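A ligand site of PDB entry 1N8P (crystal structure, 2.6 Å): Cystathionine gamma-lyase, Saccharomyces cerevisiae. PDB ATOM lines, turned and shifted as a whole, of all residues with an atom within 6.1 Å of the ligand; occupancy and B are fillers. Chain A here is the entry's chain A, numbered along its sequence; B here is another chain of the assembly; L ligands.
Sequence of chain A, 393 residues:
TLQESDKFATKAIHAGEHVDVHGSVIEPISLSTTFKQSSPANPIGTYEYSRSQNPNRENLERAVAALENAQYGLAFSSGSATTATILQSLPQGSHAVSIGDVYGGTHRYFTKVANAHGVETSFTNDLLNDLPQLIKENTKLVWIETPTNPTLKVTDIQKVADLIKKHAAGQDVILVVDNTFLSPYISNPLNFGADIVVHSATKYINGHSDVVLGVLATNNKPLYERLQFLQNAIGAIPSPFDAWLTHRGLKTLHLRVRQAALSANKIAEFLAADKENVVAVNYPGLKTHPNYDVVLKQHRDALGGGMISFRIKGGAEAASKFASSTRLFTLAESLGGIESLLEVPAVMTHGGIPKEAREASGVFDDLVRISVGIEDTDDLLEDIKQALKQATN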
ATOM      1  N   SER A  77     -33.559  -6.410  -5.364  1.00  0.00           N
ATOM      2  CA  SER A  77     -33.689  -5.614  -6.588  1.00  0.00           C
ATOM      3  C   SER A  77     -32.779  -6.094  -7.712  1.00  0.00           C
ATOM      4  O   SER A  77     -33.198  -6.223  -8.844  1.00  0.00           O
ATOM      5  CB  SER A  77     -33.363  -4.176  -6.290  1.00  0.00           C
ATOM      6  OG  SER A  77     -34.024  -3.733  -5.124  1.00  0.00           O
ATOM      7  N   SER A  78     -31.541  -6.391  -7.395  1.00  0.00           N
ATOM      8  CA  SER A  78     -30.586  -6.818  -8.415  1.00  0.00           C
ATOM      9  C   SER A  78     -29.532  -7.757  -7.856  1.00  0.00           C
ATOM     10  O   SER A  78     -29.472  -7.971  -6.636  1.00  0.00           O
ATOM     11  CB  SER A  78     -29.836  -5.591  -9.007  1.00  0.00           C
ATOM     12  OG  SER A  78     -29.550  -4.581  -8.031  1.00  0.00           O
ATOM     13  N   GLY A  79     -28.731  -8.343  -8.746  1.00  0.00           N
ATOM     14  CA  GLY A  79     -27.646  -9.155  -8.250  1.00  0.00           C
ATOM     15  C   GLY A  79     -26.888  -8.175  -7.374  1.00  0.00           C
ATOM     16  O   GLY A  79     -26.681  -8.437  -6.201  1.00  0.00           O
ATOM     17  N   SER A  80     -26.536  -7.023  -7.935  1.00  0.00           N
ATOM     18  CA  SER A  80     -25.796  -5.986  -7.228  1.00  0.00           C
ATOM     19  C   SER A  80     -26.287  -5.678  -5.816  1.00  0.00           C
ATOM     20  O   SER A  80     -25.472  -5.491  -4.905  1.00  0.00           O
ATOM     21  CB  SER A  80     -25.801  -4.701  -8.041  1.00  0.00           C
ATOM     22  OG  SER A  80     -25.174  -4.922  -9.275  1.00  0.00           O
ATOM     23  N   ALA A  81     -27.597  -5.579  -5.644  1.00  0.00           N
ATOM     24  CA  ALA A  81     -28.178  -5.294  -4.341  1.00  0.00           C
ATOM     25  C   ALA A  81     -27.932  -6.470  -3.396  1.00  0.00           C
ATOM     26  O   ALA A  81     -27.783  -6.284  -2.199  1.00  0.00           O
ATOM     27  CB  ALA A  81     -29.666  -5.070  -4.501  1.00  0.00           C
ATOM     28  N   TYR A 103     -16.984  -9.244 -12.379  1.00  0.00           N
ATOM     29  CA  TYR A 103     -17.820  -8.188 -12.960  1.00  0.00           C
ATOM     30  C   TYR A 103     -17.412  -6.950 -12.164  1.00  0.00           C
ATOM     31  O   TYR A 103     -17.046  -7.072 -10.988  1.00  0.00           O
ATOM     32  CB  TYR A 103     -19.308  -8.455 -12.675  1.00  0.00           C
ATOM     33  CG  TYR A 103     -20.232  -8.534 -13.887  1.00  0.00           C
ATOM     34  CD1 TYR A 103     -20.150  -9.587 -14.807  1.00  0.00           C
ATOM     35  CD2 TYR A 103     -21.213  -7.557 -14.102  1.00  0.00           C
ATOM     36  CE1 TYR A 103     -21.025  -9.682 -15.898  1.00  0.00           C
ATOM     37  CE2 TYR A 103     -22.101  -7.637 -15.188  1.00  0.00           C
ATOM     38  CZ  TYR A 103     -22.004  -8.697 -16.090  1.00  0.00           C
ATOM     39  OH  TYR A 103     -22.893  -8.798 -17.151  1.00  0.00           O
ATOM     40  N   ARG A 108     -17.247  -1.977  -7.762  1.00  0.00           N
ATOM     41  CA  ARG A 108     -18.204  -0.970  -7.317  1.00  0.00           C
ATOM     42  C   ARG A 108     -18.681  -1.255  -5.890  1.00  0.00           C
ATOM     43  O   ARG A 108     -18.265  -0.574  -4.934  1.00  0.00           O
ATOM     44  CB  ARG A 108     -19.422  -0.937  -8.243  1.00  0.00           C
ATOM     45  CG  ARG A 108     -19.125  -0.555  -9.662  1.00  0.00           C
ATOM     46  CD  ARG A 108     -20.409  -0.555 -10.484  1.00  0.00           C
ATOM     47  NE  ARG A 108     -21.206  -1.763 -10.259  1.00  0.00           N
ATOM     48  CZ  ARG A 108     -22.247  -2.148 -10.987  1.00  0.00           C
ATOM     49  NH1 ARG A 108     -22.648  -1.414 -12.014  1.00  0.00           N
ATOM     50  NH2 ARG A 108     -22.900  -3.264 -10.678  1.00  0.00           N
ATOM     51  N   GLU A 145     -16.384 -16.580  -8.220  1.00  0.00           N
ATOM     52  CA  GLU A 145     -17.232 -16.479  -9.390  1.00  0.00           C
ATOM     53  C   GLU A 145     -16.868 -17.725 -10.189  1.00  0.00           C
ATOM     54  O   GLU A 145     -16.156 -17.642 -11.167  1.00  0.00           O
ATOM     55  CB  GLU A 145     -16.878 -15.206 -10.141  1.00  0.00           C
ATOM     56  CG  GLU A 145     -17.854 -14.749 -11.179  1.00  0.00           C
ATOM     57  CD  GLU A 145     -17.387 -13.488 -11.867  1.00  0.00           C
ATOM     58  OE1 GLU A 145     -16.377 -13.567 -12.583  1.00  0.00           O
ATOM     59  OE2 GLU A 145     -18.013 -12.422 -11.656  1.00  0.00           O
ATOM     60  N   ASN A 149     -15.962 -14.684 -15.866  1.00  0.00           N
ATOM     61  CA  ASN A 149     -16.431 -14.007 -17.061  1.00  0.00           C
ATOM     62  C   ASN A 149     -15.288 -13.130 -17.593  1.00  0.00           C
ATOM     63  O   ASN A 149     -14.844 -12.219 -16.891  1.00  0.00           O
ATOM     64  CB  ASN A 149     -17.656 -13.197 -16.666  1.00  0.00           C
ATOM     65  CG  ASN A 149     -18.162 -12.321 -17.758  1.00  0.00           C
ATOM     66  OD1 ASN A 149     -18.451 -12.778 -18.866  1.00  0.00           O
ATOM     67  ND2 ASN A 149     -18.295 -11.045 -17.459  1.00  0.00           N
ATOM     68  N   ASP A 178     -20.746 -17.072  -6.783  1.00  0.00           N
ATOM     69  CA  ASP A 178     -21.619 -16.487  -7.805  1.00  0.00           C
ATOM     70  C   ASP A 178     -21.869 -17.589  -8.779  1.00  0.00           C
ATOM     71  O   ASP A 178     -20.978 -17.939  -9.540  1.00  0.00           O
ATOM     72  CB  ASP A 178     -20.908 -15.361  -8.553  1.00  0.00           C
ATOM     73  CG  ASP A 178     -21.866 -14.463  -9.303  1.00  0.00           C
ATOM     74  OD1 ASP A 178     -22.685 -14.958 -10.099  1.00  0.00           O
ATOM     75  OD2 ASP A 178     -21.804 -13.235  -9.094  1.00  0.00           O
ATOM     76  N   THR A 180     -24.399 -17.534 -11.097  1.00  0.00           N
ATOM     77  CA  THR A 180     -25.218 -16.986 -12.205  1.00  0.00           C
ATOM     78  C   THR A 180     -25.126 -17.719 -13.564  1.00  0.00           C
ATOM     79  O   THR A 180     -26.131 -18.225 -14.079  1.00  0.00           O
ATOM     80  CB  THR A 180     -24.895 -15.446 -12.439  1.00  0.00           C
ATOM     81  OG1 THR A 180     -25.449 -14.652 -11.358  1.00  0.00           O
ATOM     82  CG2 THR A 180     -25.456 -14.959 -13.783  1.00  0.00           C
ATOM     83  N   PHE A 181     -23.925 -17.762 -14.140  1.00  0.00           N
ATOM     84  CA  PHE A 181     -23.644 -18.412 -15.437  1.00  0.00           C
ATOM     85  C   PHE A 181     -23.959 -19.888 -15.613  1.00  0.00           C
ATOM     86  O   PHE A 181     -24.156 -20.342 -16.732  1.00  0.00           O
ATOM     87  CB  PHE A 181     -22.171 -18.233 -15.794  1.00  0.00           C
ATOM     88  CG  PHE A 181     -21.792 -16.827 -16.150  1.00  0.00           C
ATOM     89  CD1 PHE A 181     -22.576 -15.758 -15.718  1.00  0.00           C
ATOM     90  CD2 PHE A 181     -20.628 -16.578 -16.868  1.00  0.00           C
ATOM     91  CE1 PHE A 181     -22.188 -14.461 -16.000  1.00  0.00           C
ATOM     92  CE2 PHE A 181     -20.240 -15.280 -17.150  1.00  0.00           C
ATOM     93  CZ  PHE A 181     -21.029 -14.217 -16.710  1.00  0.00           C
ATOM     94  N   SER A 200     -27.722 -13.633 -10.293  1.00  0.00           N
ATOM     95  CA  SER A 200     -28.267 -12.467 -10.928  1.00  0.00           C
ATOM     96  C   SER A 200     -29.398 -13.220 -11.648  1.00  0.00           C
ATOM     97  O   SER A 200     -29.144 -13.955 -12.624  1.00  0.00           O
ATOM     98  CB  SER A 200     -27.269 -11.897 -11.904  1.00  0.00           C
ATOM     99  OG  SER A 200     -27.823 -10.775 -12.509  1.00  0.00           O
ATOM    100  N   ALA A 201     -30.622 -13.108 -11.145  1.00  0.00           N
ATOM    101  CA  ALA A 201     -31.767 -13.807 -11.710  1.00  0.00           C
ATOM    102  C   ALA A 201     -32.204 -13.217 -13.031  1.00  0.00           C
ATOM    103  O   ALA A 201     -33.162 -13.676 -13.666  1.00  0.00           O
ATOM    104  CB  ALA A 201     -32.930 -13.796 -10.696  1.00  0.00           C
ATOM    105  N   THR A 202     -31.482 -12.165 -13.424  1.00  0.00           N
ATOM    106  CA  THR A 202     -31.704 -11.457 -14.680  1.00  0.00           C
ATOM    107  C   THR A 202     -31.339 -12.376 -15.816  1.00  0.00           C
ATOM    108  O   THR A 202     -31.932 -12.364 -16.881  1.00  0.00           O
ATOM    109  CB  THR A 202     -30.798 -10.247 -14.803  1.00  0.00           C
ATOM    110  OG1 THR A 202     -31.005  -9.389 -13.675  1.00  0.00           O
ATOM    111  CG2 THR A 202     -31.077  -9.506 -16.112  1.00  0.00           C
ATOM    112  N   LYS A 203     -30.351 -13.190 -15.575  1.00  0.00           N
ATOM    113  CA  LYS A 203     -29.881 -14.061 -16.600  1.00  0.00           C
ATOM    114  C   LYS A 203     -30.677 -15.355 -16.801  1.00  0.00           C
ATOM    115  O   LYS A 203     -31.786 -15.306 -17.290  1.00  0.00           O
ATOM    116  CB  LYS A 203     -28.390 -14.334 -16.347  1.00  0.00           C
ATOM    117  CG  LYS A 203     -27.488 -13.156 -16.720  1.00  0.00           C
ATOM    118  CD  LYS A 203     -27.642 -11.934 -15.850  1.00  0.00           C
ATOM    119  CE  LYS A 203     -26.974 -10.699 -16.487  1.00  0.00           C
ATOM    120  NZ  LYS A 203     -26.475  -9.827 -15.416  1.00  0.00           N
ATOM    121  N   VAL A 212     -34.901  -7.597 -13.667  1.00  0.00           N
ATOM    122  CA  VAL A 212     -33.631  -7.417 -12.994  1.00  0.00           C
ATOM    123  C   VAL A 212     -33.988  -7.763 -11.555  1.00  0.00           C
ATOM    124  O   VAL A 212     -34.676  -7.012 -10.848  1.00  0.00           O
ATOM    125  CB  VAL A 212     -33.136  -5.968 -13.033  1.00  0.00           C
ATOM    126  CG1 VAL A 212     -32.002  -5.812 -12.073  1.00  0.00           C
ATOM    127  CG2 VAL A 212     -32.693  -5.593 -14.406  1.00  0.00           C
ATOM    128  N   LEU A 213     -33.518  -8.914 -11.118  1.00  0.00           N
ATOM    129  CA  LEU A 213     -33.764  -9.404  -9.789  1.00  0.00           C
ATOM    130  C   LEU A 213     -32.578 -10.286  -9.403  1.00  0.00           C
ATOM    131  O   LEU A 213     -31.988 -10.943 -10.271  1.00  0.00           O
ATOM    132  CB  LEU A 213     -35.066 -10.205  -9.795  1.00  0.00           C
ATOM    133  CG  LEU A 213     -35.545 -10.921  -8.546  1.00  0.00           C
ATOM    134  CD1 LEU A 213     -37.025 -10.966  -8.550  1.00  0.00           C
ATOM    135  CD2 LEU A 213     -34.987 -12.323  -8.500  1.00  0.00           C
ATOM    136  N   GLY A 214     -32.197 -10.256  -8.132  1.00  0.00           N
ATOM    137  CA  GLY A 214     -31.109 -11.103  -7.649  1.00  0.00           C
ATOM    138  C   GLY A 214     -31.587 -11.957  -6.488  1.00  0.00           C
ATOM    139  O   GLY A 214     -32.506 -11.597  -5.751  1.00  0.00           O
ATOM    140  N   SER A 334     -25.071  -8.184 -21.450  1.00  0.00           N
ATOM    141  CA  SER A 334     -25.846  -9.224 -20.774  1.00  0.00           C
ATOM    142  C   SER A 334     -25.627 -10.601 -21.368  1.00  0.00           C
ATOM    143  O   SER A 334     -24.753 -10.790 -22.223  1.00  0.00           O
ATOM    144  CB  SER A 334     -27.331  -8.922 -20.764  1.00  0.00           C
ATOM    145  OG  SER A 334     -27.974  -9.776 -19.842  1.00  0.00           O
ATOM    146  N   LEU A 335     -26.443 -11.547 -20.917  1.00  0.00           N
ATOM    147  CA  LEU A 335     -26.320 -12.935 -21.335  1.00  0.00           C
ATOM    148  C   LEU A 335     -27.381 -13.811 -20.690  1.00  0.00           C
ATOM    149  O   LEU A 335     -28.273 -13.342 -20.018  1.00  0.00           O
ATOM    150  CB  LEU A 335     -24.972 -13.458 -20.888  1.00  0.00           C
ATOM    151  CG  LEU A 335     -24.940 -13.402 -19.352  1.00  0.00           C
ATOM    152  CD1 LEU A 335     -24.817 -14.795 -18.760  1.00  0.00           C
ATOM    153  CD2 LEU A 335     -23.812 -12.521 -18.907  1.00  0.00           C
ATOM    154  N   TYR B  49     -28.288  -1.149 -20.568  1.00  0.00           N
ATOM    155  CA  TYR B  49     -28.672  -2.148 -19.573  1.00  0.00           C
ATOM    156  C   TYR B  49     -29.730  -1.571 -18.639  1.00  0.00           C
ATOM    157  O   TYR B  49     -29.525  -0.493 -18.068  1.00  0.00           O
ATOM    158  CB  TYR B  49     -27.430  -2.600 -18.784  1.00  0.00           C
ATOM    159  CG  TYR B  49     -27.626  -3.850 -17.955  1.00  0.00           C
ATOM    160  CD1 TYR B  49     -27.932  -5.059 -18.571  1.00  0.00           C
ATOM    161  CD2 TYR B  49     -27.539  -3.812 -16.573  1.00  0.00           C
ATOM    162  CE1 TYR B  49     -28.161  -6.196 -17.813  1.00  0.00           C
ATOM    163  CE2 TYR B  49     -27.770  -4.925 -15.811  1.00  0.00           C
ATOM    164  CZ  TYR B  49     -28.084  -6.113 -16.430  1.00  0.00           C
ATOM    165  OH  TYR B  49     -28.374  -7.214 -15.651  1.00  0.00           O
ATOM    166  N   ARG B  51     -30.868  -1.951 -15.477  1.00  0.00           N
ATOM    167  CA  ARG B  51     -30.526  -1.441 -14.143  1.00  0.00           C
ATOM    168  C   ARG B  51     -29.733  -0.158 -14.203  1.00  0.00           C
ATOM    169  O   ARG B  51     -29.819   0.665 -13.306  1.00  0.00           O
ATOM    170  CB  ARG B  51     -29.712  -2.456 -13.335  1.00  0.00           C
ATOM    171  CG  ARG B  51     -29.028  -1.828 -12.118  1.00  0.00           C
ATOM    172  CD  ARG B  51     -28.512  -2.872 -11.178  1.00  0.00           C
ATOM    173  NE  ARG B  51     -27.721  -3.879 -11.861  1.00  0.00           N
ATOM    174  CZ  ARG B  51     -26.507  -3.680 -12.384  1.00  0.00           C
ATOM    175  NH1 ARG B  51     -25.935  -2.482 -12.308  1.00  0.00           N
ATOM    176  NH2 ARG B  51     -25.870  -4.686 -12.976  1.00  0.00           N
ATOM    177  N   GLY B 235     -27.557  -1.196  -6.789  1.00  0.00           N
ATOM    178  CA  GLY B 235     -28.684  -1.718  -7.544  1.00  0.00           C
ATOM    179  C   GLY B 235     -30.042  -1.757  -6.876  1.00  0.00           C
ATOM    180  O   GLY B 235     -30.888  -2.541  -7.304  1.00  0.00           O
HETATM  181  N1  LIG L   1     -22.994 -10.770 -11.666  1.00  0.00           N
HETATM  182  C1  LIG L   1     -22.845 -11.541 -12.801  1.00  0.00           C
HETATM  183  C2  LIG L   1     -21.916 -12.734 -12.658  1.00  0.00           C
HETATM  184  C3  LIG L   1     -23.609 -11.096 -14.004  1.00  0.00           C
HETATM  185  O1  LIG L   1     -23.430 -11.946 -15.055  1.00  0.00           O
HETATM  186  C4  LIG L   1     -24.433  -9.930 -13.955  1.00  0.00           C
HETATM  187  C5  LIG L   1     -25.177  -9.475 -15.180  1.00  0.00           C
HETATM  188  C6  LIG L   1     -24.495  -9.208 -12.658  1.00  0.00           C
HETATM  189  C7  LIG L   1     -23.779  -9.638 -11.562  1.00  0.00           C
HETATM  190  C8  LIG L   1     -25.436  -7.996 -12.558  1.00  0.00           C
HETATM  191  O2  LIG L   1     -26.727  -8.320 -12.075  1.00  0.00           O
HETATM  192  P1  LIG L   1     -27.778  -7.189 -11.837  1.00  0.00           P
HETATM  193  O3  LIG L   1     -28.997  -7.920 -11.582  1.00  0.00           O
HETATM  194  O4  LIG L   1     -27.844  -6.400 -13.128  1.00  0.00           O
HETATM  195  O5  LIG L   1     -27.207  -6.421 -10.749  1.00  0.00           O
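Residues that only touch the ligand: Phe 181, Tyr 103, Ser 78, Asp 178, Val 212, Thr 180 and Leu 335.
Hydrophobic or aromatic side chains that line the ligand: Tyr 103, Phe 181, Val 212, Leu 335 and Tyr 49 of chain B.
The side-chain amino group (NZ) of Lys 203 is covalently linked to a carbon (C5) of the ligand (1.4 Å).
An oxygen (O4) of the ligand is in salt-bridge range of the guanidinium group of Arg 51 of chain B (2.6 Å).
O4 of the ligand sits at hydrogen-bond distance from OH of Tyr 49 of chain B (2.7 Å).
O2 of the ligand is in hydrogen-bond range of OG of Ser 200 (2.7 Å).
The backbone NH (N) of Gly 79 lies within hydrogen-bond range of an oxygen (O3) of the ligand.
An oxygen (O5) of the ligand is in hydrogen-bond range of the backbone NH (N) of Ser 80 (3.0 Å).
OG of Ser 80 is in hydrogen-bond range of O5 of the ligand (2.9 Å).
An oxygen (O3) of the ligand is in hydrogen-bond range of the side-chain hydroxyl of Thr 202, 3.3 Å away.
The side-chain hydroxyl of Tyr 49 of chain B sits at hydrogen-bond distance from the side-chain amino group of Lys 203 (3.2 Å).
The side-chain hydroxyl (OG) of Ser 200 lies within hydrogen-bond range of the side-chain amino group (NZ) of Lys 203, 3.3 Å away.
The side-chain hydroxyl (OG1) of Thr 180 lies within hydrogen-bond range of the backbone NH (N) of Ser 200 (2.7 Å).
The side-chain hydroxyl (OG) of Ser 80 is in hydrogen-bond range of the guanidinium group (NH2) of Arg 108 (3.1 Å).
The backbone carbonyl oxygen (O) of Leu 213 is in hydrogen-bond range of the backbone NH (N) of Thr 202, at 3.4 Å.
The backbone NH (N) of Ala 81 sits at hydrogen-bond distance from the side-chain hydroxyl (OG) of Ser 78, at 3.2 Å.
The side-chain hydroxyl (OG) of Ser 78 sits at hydrogen-bond distance from the backbone carbonyl oxygen (O) of Gly 235 of chain B, at 2.5 Å.
The side-chain carboxylate (OD1) of Asp 178 is in hydrogen-bond range of the side-chain hydroxyl (OG1) of Thr 180, at 3.1 Å.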
